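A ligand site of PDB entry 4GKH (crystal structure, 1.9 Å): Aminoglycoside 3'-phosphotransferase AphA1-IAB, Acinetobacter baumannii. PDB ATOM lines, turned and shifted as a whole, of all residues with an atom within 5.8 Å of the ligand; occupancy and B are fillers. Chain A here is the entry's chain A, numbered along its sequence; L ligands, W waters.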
ATOM      1  N   GLY A  35      -7.617  -5.981 -28.943  1.00  0.00           N
ATOM      2  CA  GLY A  35      -6.896  -4.862 -28.365  1.00  0.00           C
ATOM      3  C   GLY A  35      -7.348  -3.447 -28.713  1.00  0.00           C
ATOM      4  O   GLY A  35      -7.870  -3.174 -29.803  1.00  0.00           O
ATOM      5  N   GLN A  36      -7.084  -2.529 -27.775  1.00  0.00           N
ATOM      6  CA  GLN A  36      -7.607  -1.159 -27.791  1.00  0.00           C
ATOM      7  C   GLN A  36      -7.146  -0.267 -28.957  1.00  0.00           C
ATOM      8  O   GLN A  36      -7.966   0.348 -29.647  1.00  0.00           O
ATOM      9  CB  GLN A  36      -7.265  -0.483 -26.460  1.00  0.00           C
ATOM     10  CG  GLN A  36      -7.750   0.942 -26.314  1.00  0.00           C
ATOM     11  CD  GLN A  36      -7.263   1.584 -25.029  1.00  0.00           C
ATOM     12  OE1 GLN A  36      -6.149   2.105 -24.956  1.00  0.00           O
ATOM     13  NE2 GLN A  36      -8.092   1.523 -24.004  1.00  0.00           N
ATOM     14  N   SER A  37      -5.830  -0.158 -29.147  1.00  0.00           N
ATOM     15  CA  SER A  37      -5.292   0.650 -30.241  1.00  0.00           C
ATOM     16  C   SER A  37      -5.119  -0.193 -31.497  1.00  0.00           C
ATOM     17  O   SER A  37      -5.496  -1.362 -31.519  1.00  0.00           O
ATOM     18  CB  SER A  37      -3.958   1.284 -29.837  1.00  0.00           C
ATOM     19  OG  SER A  37      -2.972   0.295 -29.575  1.00  0.00           O
ATOM     20  N   ARG A 156      -9.321  13.124 -34.226  1.00  0.00           N
ATOM     21  CA  ARG A 156      -9.631  11.842 -34.846  1.00  0.00           C
ATOM     22  C   ARG A 156     -10.684  11.977 -35.934  1.00  0.00           C
ATOM     23  O   ARG A 156     -10.555  11.387 -37.006  1.00  0.00           O
ATOM     24  CB  ARG A 156     -10.039  10.800 -33.794  1.00  0.00           C
ATOM     25  CG  ARG A 156      -8.819  10.286 -33.015  1.00  0.00           C
ATOM     26  CD  ARG A 156      -9.169   9.213 -32.031  1.00  0.00           C
ATOM     27  NE  ARG A 156     -10.086   8.224 -32.572  1.00  0.00           N
ATOM     28  CZ  ARG A 156      -9.722   7.174 -33.289  1.00  0.00           C
ATOM     29  NH1 ARG A 156     -10.645   6.310 -33.714  1.00  0.00           N
ATOM     30  NH2 ARG A 156      -8.449   6.961 -33.577  1.00  0.00           N
ATOM     31  N   ASP A 163     -14.562   5.373 -36.654  1.00  0.00           N
ATOM     32  CA  ASP A 163     -15.273   4.257 -37.282  1.00  0.00           C
ATOM     33  C   ASP A 163     -16.777   4.471 -37.253  1.00  0.00           C
ATOM     34  O   ASP A 163     -17.419   4.097 -36.277  1.00  0.00           O
ATOM     35  CB  ASP A 163     -14.932   2.957 -36.562  1.00  0.00           C
ATOM     36  CG  ASP A 163     -15.538   1.718 -37.236  1.00  0.00           C
ATOM     37  OD1 ASP A 163     -16.273   1.847 -38.242  1.00  0.00           O
ATOM     38  OD2 ASP A 163     -15.272   0.602 -36.740  1.00  0.00           O
ATOM     39  N   ASP A 166     -19.337   1.650 -36.453  1.00  0.00           N
ATOM     40  CA  ASP A 166     -19.336   1.019 -35.130  1.00  0.00           C
ATOM     41  C   ASP A 166     -20.121   1.817 -34.080  1.00  0.00           C
ATOM     42  O   ASP A 166     -19.939   1.611 -32.889  1.00  0.00           O
ATOM     43  CB  ASP A 166     -17.879   0.789 -34.649  1.00  0.00           C
ATOM     44  CG  ASP A 166     -17.767  -0.251 -33.539  1.00  0.00           C
ATOM     45  OD1 ASP A 166     -18.619  -1.171 -33.484  1.00  0.00           O
ATOM     46  OD2 ASP A 166     -16.822  -0.152 -32.724  1.00  0.00           O
ATOM     47  N   PHE A 167     -20.962   2.757 -34.518  1.00  0.00           N
ATOM     48  CA  PHE A 167     -21.724   3.557 -33.551  1.00  0.00           C
ATOM     49  C   PHE A 167     -22.778   2.689 -32.852  1.00  0.00           C
ATOM     50  O   PHE A 167     -23.178   1.649 -33.371  1.00  0.00           O
ATOM     51  CB  PHE A 167     -22.458   4.708 -34.247  1.00  0.00           C
ATOM     52  CG  PHE A 167     -21.558   5.786 -34.803  1.00  0.00           C
ATOM     53  CD1 PHE A 167     -20.252   5.935 -34.351  1.00  0.00           C
ATOM     54  CD2 PHE A 167     -22.019   6.642 -35.803  1.00  0.00           C
ATOM     55  CE1 PHE A 167     -19.441   6.940 -34.856  1.00  0.00           C
ATOM     56  CE2 PHE A 167     -21.208   7.638 -36.329  1.00  0.00           C
ATOM     57  CZ  PHE A 167     -19.929   7.782 -35.860  1.00  0.00           C
ATOM     58  N   ASP A 168     -23.233   3.133 -31.673  1.00  0.00           N
ATOM     59  CA  ASP A 168     -24.360   2.486 -30.990  1.00  0.00           C
ATOM     60  C   ASP A 168     -25.659   2.547 -31.800  1.00  0.00           C
ATOM     61  O   ASP A 168     -25.772   3.304 -32.759  1.00  0.00           O
ATOM     62  CB  ASP A 168     -24.600   3.138 -29.625  1.00  0.00           C
ATOM     63  CG  ASP A 168     -23.439   2.948 -28.677  1.00  0.00           C
ATOM     64  OD1 ASP A 168     -22.809   1.864 -28.688  1.00  0.00           O
ATOM     65  OD2 ASP A 168     -23.167   3.904 -27.907  1.00  0.00           O
ATOM     66  N   ASP A 169     -26.667   1.765 -31.387  1.00  0.00           N
ATOM     67  CA  ASP A 169     -27.899   1.678 -32.174  1.00  0.00           C
ATOM     68  C   ASP A 169     -28.634   3.015 -32.267  1.00  0.00           C
ATOM     69  O   ASP A 169     -29.234   3.318 -33.309  1.00  0.00           O
ATOM     70  CB  ASP A 169     -28.833   0.601 -31.605  1.00  0.00           C
ATOM     71  CG  ASP A 169     -28.346  -0.810 -31.894  1.00  0.00           C
ATOM     72  OD1 ASP A 169     -27.662  -1.000 -32.923  1.00  0.00           O
ATOM     73  OD2 ASP A 169     -28.659  -1.736 -31.107  1.00  0.00           O
ATOM     74  N   ASP A 199     -11.315   2.730 -20.713  1.00  0.00           N
ATOM     75  CA  ASP A 199     -11.994   1.777 -21.594  1.00  0.00           C
ATOM     76  C   ASP A 199     -12.471   0.578 -20.753  1.00  0.00           C
ATOM     77  O   ASP A 199     -12.050  -0.545 -20.965  1.00  0.00           O
ATOM     78  CB  ASP A 199     -11.059   1.354 -22.745  1.00  0.00           C
ATOM     79  CG  ASP A 199     -11.786   0.637 -23.869  1.00  0.00           C
ATOM     80  OD1 ASP A 199     -13.029   0.525 -23.823  1.00  0.00           O
ATOM     81  OD2 ASP A 199     -11.107   0.200 -24.823  1.00  0.00           O
ATOM     82  N   SER A 201     -14.519  -1.782 -20.407  1.00  0.00           N
ATOM     83  CA  SER A 201     -15.470  -2.618 -21.105  1.00  0.00           C
ATOM     84  C   SER A 201     -15.363  -4.059 -20.610  1.00  0.00           C
ATOM     85  O   SER A 201     -14.431  -4.412 -19.913  1.00  0.00           O
ATOM     86  CB  SER A 201     -15.186  -2.594 -22.604  1.00  0.00           C
ATOM     87  OG  SER A 201     -14.043  -3.399 -22.871  1.00  0.00           O
ATOM     88  N   ASP A 203     -14.428  -6.482 -22.292  1.00  0.00           N
ATOM     89  CA  ASP A 203     -13.268  -7.144 -22.887  1.00  0.00           C
ATOM     90  C   ASP A 203     -11.985  -6.864 -22.102  1.00  0.00           C
ATOM     91  O   ASP A 203     -10.971  -7.523 -22.319  1.00  0.00           O
ATOM     92  CB  ASP A 203     -13.051  -6.688 -24.329  1.00  0.00           C
ATOM     93  CG  ASP A 203     -14.250  -6.917 -25.198  1.00  0.00           C
ATOM     94  OD1 ASP A 203     -14.923  -7.957 -25.023  1.00  0.00           O
ATOM     95  OD2 ASP A 203     -14.532  -6.049 -26.059  1.00  0.00           O
ATOM     96  N   ASN A 204     -12.024  -5.888 -21.200  1.00  0.00           N
ATOM     97  CA  ASN A 204     -10.772  -5.429 -20.554  1.00  0.00           C
ATOM     98  C   ASN A 204     -10.644  -5.761 -19.078  1.00  0.00           C
ATOM     99  O   ASN A 204      -9.741  -5.263 -18.401  1.00  0.00           O
ATOM    100  CB  ASN A 204     -10.597  -3.933 -20.750  1.00  0.00           C
ATOM    101  CG  ASN A 204     -10.195  -3.590 -22.168  1.00  0.00           C
ATOM    102  OD1 ASN A 204      -9.612  -4.410 -22.865  1.00  0.00           O
ATOM    103  ND2 ASN A 204     -10.509  -2.366 -22.585  1.00  0.00           N
ATOM    104  N   ARG A 220      -5.663   4.622 -21.715  1.00  0.00           N
ATOM    105  CA  ARG A 220      -6.456   5.848 -21.549  1.00  0.00           C
ATOM    106  C   ARG A 220      -6.677   6.219 -20.073  1.00  0.00           C
ATOM    107  O   ARG A 220      -7.481   7.103 -19.757  1.00  0.00           O
ATOM    108  CB  ARG A 220      -7.819   5.695 -22.275  1.00  0.00           C
ATOM    109  CG  ARG A 220      -7.690   5.594 -23.818  1.00  0.00           C
ATOM    110  CD  ARG A 220      -9.038   5.266 -24.558  1.00  0.00           C
ATOM    111  NE  ARG A 220      -8.775   5.143 -25.996  1.00  0.00           N
ATOM    112  CZ  ARG A 220      -9.379   4.292 -26.833  1.00  0.00           C
ATOM    113  NH1 ARG A 220      -9.040   4.275 -28.117  1.00  0.00           N
ATOM    114  NH2 ARG A 220     -10.335   3.470 -26.393  1.00  0.00           N
ATOM    115  N   ASN A 235     -22.919   0.353 -21.245  1.00  0.00           N
ATOM    116  CA  ASN A 235     -23.207   0.099 -22.650  1.00  0.00           C
ATOM    117  C   ASN A 235     -23.007  -1.393 -22.982  1.00  0.00           C
ATOM    118  O   ASN A 235     -23.883  -2.022 -23.604  1.00  0.00           O
ATOM    119  CB  ASN A 235     -22.322   0.986 -23.551  1.00  0.00           C
ATOM    120  CG  ASN A 235     -22.806   1.009 -25.000  1.00  0.00           C
ATOM    121  OD1 ASN A 235     -24.002   1.020 -25.262  1.00  0.00           O
ATOM    122  ND2 ASN A 235     -21.874   1.021 -25.937  1.00  0.00           N
ATOM    123  N   CYS A 236     -21.902  -1.962 -22.518  1.00  0.00           N
ATOM    124  CA  CYS A 236     -21.611  -3.387 -22.751  1.00  0.00           C
ATOM    125  C   CYS A 236     -22.687  -4.286 -22.200  1.00  0.00           C
ATOM    126  O   CYS A 236     -23.138  -5.235 -22.868  1.00  0.00           O
ATOM    127  CB  CYS A 236     -20.284  -3.765 -22.089  1.00  0.00           C
ATOM    128  SG  CYS A 236     -18.871  -3.036 -22.959  1.00  0.00           S
ATOM    129  N   LEU A 237     -23.098  -3.990 -20.974  1.00  0.00           N
ATOM    130  CA  LEU A 237     -24.125  -4.795 -20.302  1.00  0.00           C
ATOM    131  C   LEU A 237     -25.467  -4.728 -20.998  1.00  0.00           C
ATOM    132  O   LEU A 237     -26.280  -5.639 -20.882  1.00  0.00           O
ATOM    133  CB  LEU A 237     -24.241  -4.366 -18.841  1.00  0.00           C
ATOM    134  CG  LEU A 237     -23.043  -4.702 -17.960  1.00  0.00           C
ATOM    135  CD1 LEU A 237     -23.185  -4.094 -16.553  1.00  0.00           C
ATOM    136  CD2 LEU A 237     -22.871  -6.215 -17.872  1.00  0.00           C
ATOM    137  N   GLY A 238     -25.704  -3.656 -21.752  1.00  0.00           N
ATOM    138  CA  GLY A 238     -26.920  -3.519 -22.526  1.00  0.00           C
ATOM    139  C   GLY A 238     -27.080  -4.584 -23.587  1.00  0.00           C
ATOM    140  O   GLY A 238     -28.163  -4.779 -24.122  1.00  0.00           O
ATOM    141  N   GLU A 239     -25.987  -5.292 -23.894  1.00  0.00           N
ATOM    142  CA  GLU A 239     -26.088  -6.416 -24.825  1.00  0.00           C
ATOM    143  C   GLU A 239     -26.753  -7.619 -24.156  1.00  0.00           C
ATOM    144  O   GLU A 239     -27.247  -8.519 -24.852  1.00  0.00           O
ATOM    145  CB  GLU A 239     -24.698  -6.782 -25.381  1.00  0.00           C
ATOM    146  CG  GLU A 239     -24.761  -7.570 -26.701  1.00  0.00           C
ATOM    147  CD  GLU A 239     -23.380  -7.877 -27.308  1.00  0.00           C
ATOM    148  OE1 GLU A 239     -23.336  -8.593 -28.355  1.00  0.00           O
ATOM    149  OE2 GLU A 239     -22.360  -7.405 -26.760  1.00  0.00           O
ATOM    150  N   ASP A 269     -17.376   8.170 -26.603  1.00  0.00           N
ATOM    151  CA  ASP A 269     -16.693   6.927 -26.949  1.00  0.00           C
ATOM    152  C   ASP A 269     -16.891   6.516 -28.405  1.00  0.00           C
ATOM    153  O   ASP A 269     -16.117   5.707 -28.922  1.00  0.00           O
ATOM    154  CB  ASP A 269     -17.059   5.765 -25.989  1.00  0.00           C
ATOM    155  CG  ASP A 269     -16.007   4.650 -25.983  1.00  0.00           C
ATOM    156  OD1 ASP A 269     -14.809   4.950 -25.885  1.00  0.00           O
ATOM    157  OD2 ASP A 269     -16.380   3.460 -26.059  1.00  0.00           O
ATOM    158  N   GLU A 270     -17.892   7.086 -29.073  1.00  0.00           N
ATOM    159  CA  GLU A 270     -18.100   6.838 -30.518  1.00  0.00           C
ATOM    160  C   GLU A 270     -16.876   7.248 -31.338  1.00  0.00           C
ATOM    161  O   GLU A 270     -16.628   6.731 -32.430  1.00  0.00           O
ATOM    162  CB  GLU A 270     -19.336   7.568 -31.060  1.00  0.00           C
ATOM    163  CG  GLU A 270     -20.673   7.210 -30.397  1.00  0.00           C
ATOM    164  CD  GLU A 270     -21.153   5.793 -30.716  1.00  0.00           C
ATOM    165  OE1 GLU A 270     -20.324   4.867 -30.818  1.00  0.00           O
ATOM    166  OE2 GLU A 270     -22.389   5.606 -30.847  1.00  0.00           O
ATOM    167  N   PHE A 271     -16.117   8.190 -30.798  1.00  0.00           N
ATOM    168  CA  PHE A 271     -14.988   8.789 -31.523  1.00  0.00           C
ATOM    169  C   PHE A 271     -13.667   8.009 -31.417  1.00  0.00           C
ATOM    170  O   PHE A 271     -12.680   8.352 -32.099  1.00  0.00           O
ATOM    171  CB  PHE A 271     -14.789  10.236 -31.051  1.00  0.00           C
ATOM    172  CG  PHE A 271     -15.907  11.160 -31.482  1.00  0.00           C
ATOM    173  CD1 PHE A 271     -17.055  11.286 -30.708  1.00  0.00           C
ATOM    174  CD2 PHE A 271     -15.823  11.843 -32.690  1.00  0.00           C
ATOM    175  CE1 PHE A 271     -18.095  12.119 -31.117  1.00  0.00           C
ATOM    176  CE2 PHE A 271     -16.860  12.674 -33.112  1.00  0.00           C
ATOM    177  CZ  PHE A 271     -18.002  12.813 -32.324  1.00  0.00           C
ATOM    178  N   PHE A 272     -13.656   6.976 -30.586  1.00  0.00           N
ATOM    179  CA  PHE A 272     -12.418   6.273 -30.255  1.00  0.00           C
ATOM    180  C   PHE A 272     -12.429   4.815 -30.685  1.00  0.00           C
ATOM    181  O   PHE A 272     -11.426   4.111 -30.511  1.00  0.00           O
ATOM    182  CB  PHE A 272     -12.093   6.450 -28.767  1.00  0.00           C
ATOM    183  CG  PHE A 272     -11.828   7.889 -28.403  1.00  0.00           C
ATOM    184  CD1 PHE A 272     -10.555   8.428 -28.560  1.00  0.00           C
ATOM    185  CD2 PHE A 272     -12.852   8.711 -27.975  1.00  0.00           C
ATOM    186  CE1 PHE A 272     -10.297   9.742 -28.248  1.00  0.00           C
ATOM    187  CE2 PHE A 272     -12.606  10.055 -27.671  1.00  0.00           C
ATOM    188  CZ  PHE A 272     -11.322  10.573 -27.800  1.00  0.00           C
ATOM    189  OXT PHE A 272     -13.420   4.334 -31.223  1.00  0.00           O
HETATM  190  C1  LIG L   1     -14.405  -0.616 -29.498  1.00  0.00           C
HETATM  191  C2  LIG L   1     -13.505  -1.224 -28.448  1.00  0.00           C
HETATM  192  C3  LIG L   1     -12.417  -0.263 -27.998  1.00  0.00           C
HETATM  193  C4  LIG L   1     -11.583   0.128 -29.218  1.00  0.00           C
HETATM  194  C5  LIG L   1     -12.503   0.799 -30.219  1.00  0.00           C
HETATM  195  C6  LIG L   1     -11.616   1.131 -31.422  1.00  0.00           C
HETATM  196  C7  LIG L   1     -19.054   1.895 -29.416  1.00  0.00           C
HETATM  197  C8  LIG L   1     -18.788   0.436 -29.693  1.00  0.00           C
HETATM  198  C9  LIG L   1     -17.468   0.054 -28.995  1.00  0.00           C
HETATM  199  C10 LIG L   1     -16.285   0.875 -29.563  1.00  0.00           C
HETATM  200  C11 LIG L   1     -16.593   2.359 -29.235  1.00  0.00           C
HETATM  201  C12 LIG L   1     -17.893   2.752 -29.922  1.00  0.00           C
HETATM  202  C13 LIG L   1     -20.202  -1.576 -29.765  1.00  0.00           C
HETATM  203  C14 LIG L   1     -21.728  -1.688 -29.694  1.00  0.00           C
HETATM  204  C15 LIG L   1     -22.294  -1.737 -28.293  1.00  0.00           C
HETATM  205  C16 LIG L   1     -21.688  -2.925 -27.578  1.00  0.00           C
HETATM  206  C17 LIG L   1     -20.169  -2.722 -27.571  1.00  0.00           C
HETATM  207  C18 LIG L   1     -19.419  -3.760 -26.700  1.00  0.00           C
HETATM  208  N1  LIG L   1     -12.412   1.797 -32.456  1.00  0.00           N
HETATM  209  N2  LIG L   1     -15.487   3.192 -29.765  1.00  0.00           N
HETATM  210  N3  LIG L   1     -20.318   2.207 -30.131  1.00  0.00           N
HETATM  211  N4  LIG L   1     -23.748  -1.902 -28.334  1.00  0.00           N
HETATM  212  O1  LIG L   1     -13.552  -0.133 -30.597  1.00  0.00           O
HETATM  213  O2  LIG L   1     -14.312  -1.616 -27.324  1.00  0.00           O
HETATM  214  O3  LIG L   1     -11.606  -0.948 -27.038  1.00  0.00           O
HETATM  215  O4  LIG L   1     -10.564   1.069 -28.850  1.00  0.00           O
HETATM  216  O5  LIG L   1     -15.053   0.517 -28.907  1.00  0.00           O
HETATM  217  O6  LIG L   1     -17.243  -1.377 -29.050  1.00  0.00           O
HETATM  218  O7  LIG L   1     -19.945  -0.300 -29.201  1.00  0.00           O
HETATM  219  O8  LIG L   1     -19.661  -2.641 -28.935  1.00  0.00           O
HETATM  220  O9  LIG L   1     -22.240  -0.594 -30.463  1.00  0.00           O
HETATM  221  O10 LIG L   1     -22.175  -2.937 -26.245  1.00  0.00           O
HETATM  222  O11 LIG L   1     -18.022  -3.373 -26.612  1.00  0.00           O
HETATM  223  O   HOH W   1     -10.521  -3.828 -25.641  1.00  0.00           O
HETATM  224  O   HOH W   2     -26.240  -0.270 -29.399  1.00  0.00           O
HETATM  225  O   HOH W   3     -13.274  -3.088 -25.340  1.00  0.00           O
HETATM  226  O   HOH W   4     -13.880  -0.312 -33.837  1.00  0.00           O
HETATM  227  O   HOH W   5     -24.530  -0.959 -32.883  1.00  0.00           O
HETATM  228  O   HOH W   6     -17.141  -1.280 -25.563  1.00  0.00           O
HETATM  229  O   HOH W   7     -15.463  -4.252 -28.754  1.00  0.00           O
HETATM  230  O   HOH W   8     -13.436   3.157 -27.686  1.00  0.00           O
HETATM  231  O   HOH W   9     -21.097  -1.392 -33.167  1.00  0.00           O
HETATM  232  O   HOH W  10     -14.946   1.008 -25.775  1.00  0.00           O
HETATM  233  O   HOH W  11     -11.078   3.043 -34.581  1.00  0.00           O
HETATM  234  O   HOH W  12     -15.362   2.460 -32.658  1.00  0.00           O
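OD2 of Asp 199 is in hydrogen-bond range of O3 of the ligand (2.5 Å).
A nitrogen (N2) of the ligand is in hydrogen-bond range of the backbone carbonyl oxygen of Asp 269, 2.7 Å away.
The side-chain carboxylate (OD2) of Asp 269 lies within salt-bridge range of a nitrogen (N2) of the ligand.
N3 of the ligand lies within salt-bridge range of OE1 of Glu 270, 2.7 Å away.
OXT of Phe 272 lies within salt-bridge range of N2 of the ligand (2.8 Å).
An oxygen (O4) of the ligand lies within hydrogen-bond range of the backbone carbonyl oxygen (O) of Gln 36 (2.8 Å).
O of Asp 166 is in hydrogen-bond range of N3 of the ligand (2.8 Å).
The backbone NH of Asp 168 lies close to a nitrogen (N3) of the ligand, 3.4 Å away.
The side-chain carboxylate of Asp 168 lies within salt-bridge range of a nitrogen (N3) of the ligand (2.9 Å).
O of Asn 235 lies within hydrogen-bond range of O10 of the ligand (3.3 Å).
The guanidinium group of Arg 220 is in hydrogen-bond range of an oxygen (O4) of the ligand, 3.4 Å away.
The side-chain sulfur (SG) of Cys 236 sits at hydrogen-bond distance from an oxygen (O11) of the ligand (3.8 Å).
The side-chain carboxylate of Asp 199 sits close to the side-chain amide nitrogen of Gln 36 (3.4 Å).
The guanidinium group of Arg 220 is in salt-bridge range of the side-chain carboxylate of Asp 199 (3.7 Å).
The backbone carbonyl oxygen of Asp 199 sits at hydrogen-bond distance from the side-chain amide nitrogen of Asn 204, 2.9 Å away.
N of Asp 168 lies within hydrogen-bond range of OE2 of Glu 270 (2.7 Å).
NH1 of Arg 220 lies within salt-bridge range of O of Phe 272, 3.4 Å away.
NH1 of Arg 156 is in salt-bridge range of O of Phe 272 (3.96 Å).
The side-chain carboxylate (OD1) of Asp 168 sits at hydrogen-bond distance from the side-chain amide nitrogen (ND2) of Asn 235, 3.0 Å away.
Phe 167 touches the ligand.
Within 4 Å of the ligand: Gln 36, Asp 166, Phe 167, Asp 168, Asp 199, Arg 220, Asn 235, Cys 236, Asp 269, Glu 270 and Phe 272.
The nearest printed residue that does not touch the ligand is Asp 203 (4.4 Å).
Water W3 lies within hydrogen-bond range of the side-chain hydroxyl (OG) of Ser 201, an oxygen (O2) of the ligand and the side-chain carboxylate (OD2) of Asp 203.
Water W8 lies within hydrogen-bond range of the side-chain carboxylate (OD1) of Asp 269 (2.9 Å), a nitrogen (N2) of the ligand (2.9 Å) and the guanidinium group (NH2) of Arg 220 (3.4 Å).
Water W10 lies within hydrogen-bond range of the side-chain carboxylate (OD1) of Asp 199 (2.8 Å), the side-chain carboxylate (OD2) of Asp 269 (2.9 Å) and an oxygen (O2) of the ligand (3.1 Å).
Water W2 bridges N of Asp 169 (2.9 Å) and N4 of the ligand (3.2 Å).
Water W5 lies within hydrogen-bond range of the backbone carbonyl oxygen of Phe 167, the side-chain carboxylate of Asp 169 and an oxygen (O9) of the ligand.
Water W1 bridges OD1 of Asn 204 (3.0 Å) and O3 of the ligand (3.4 Å).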
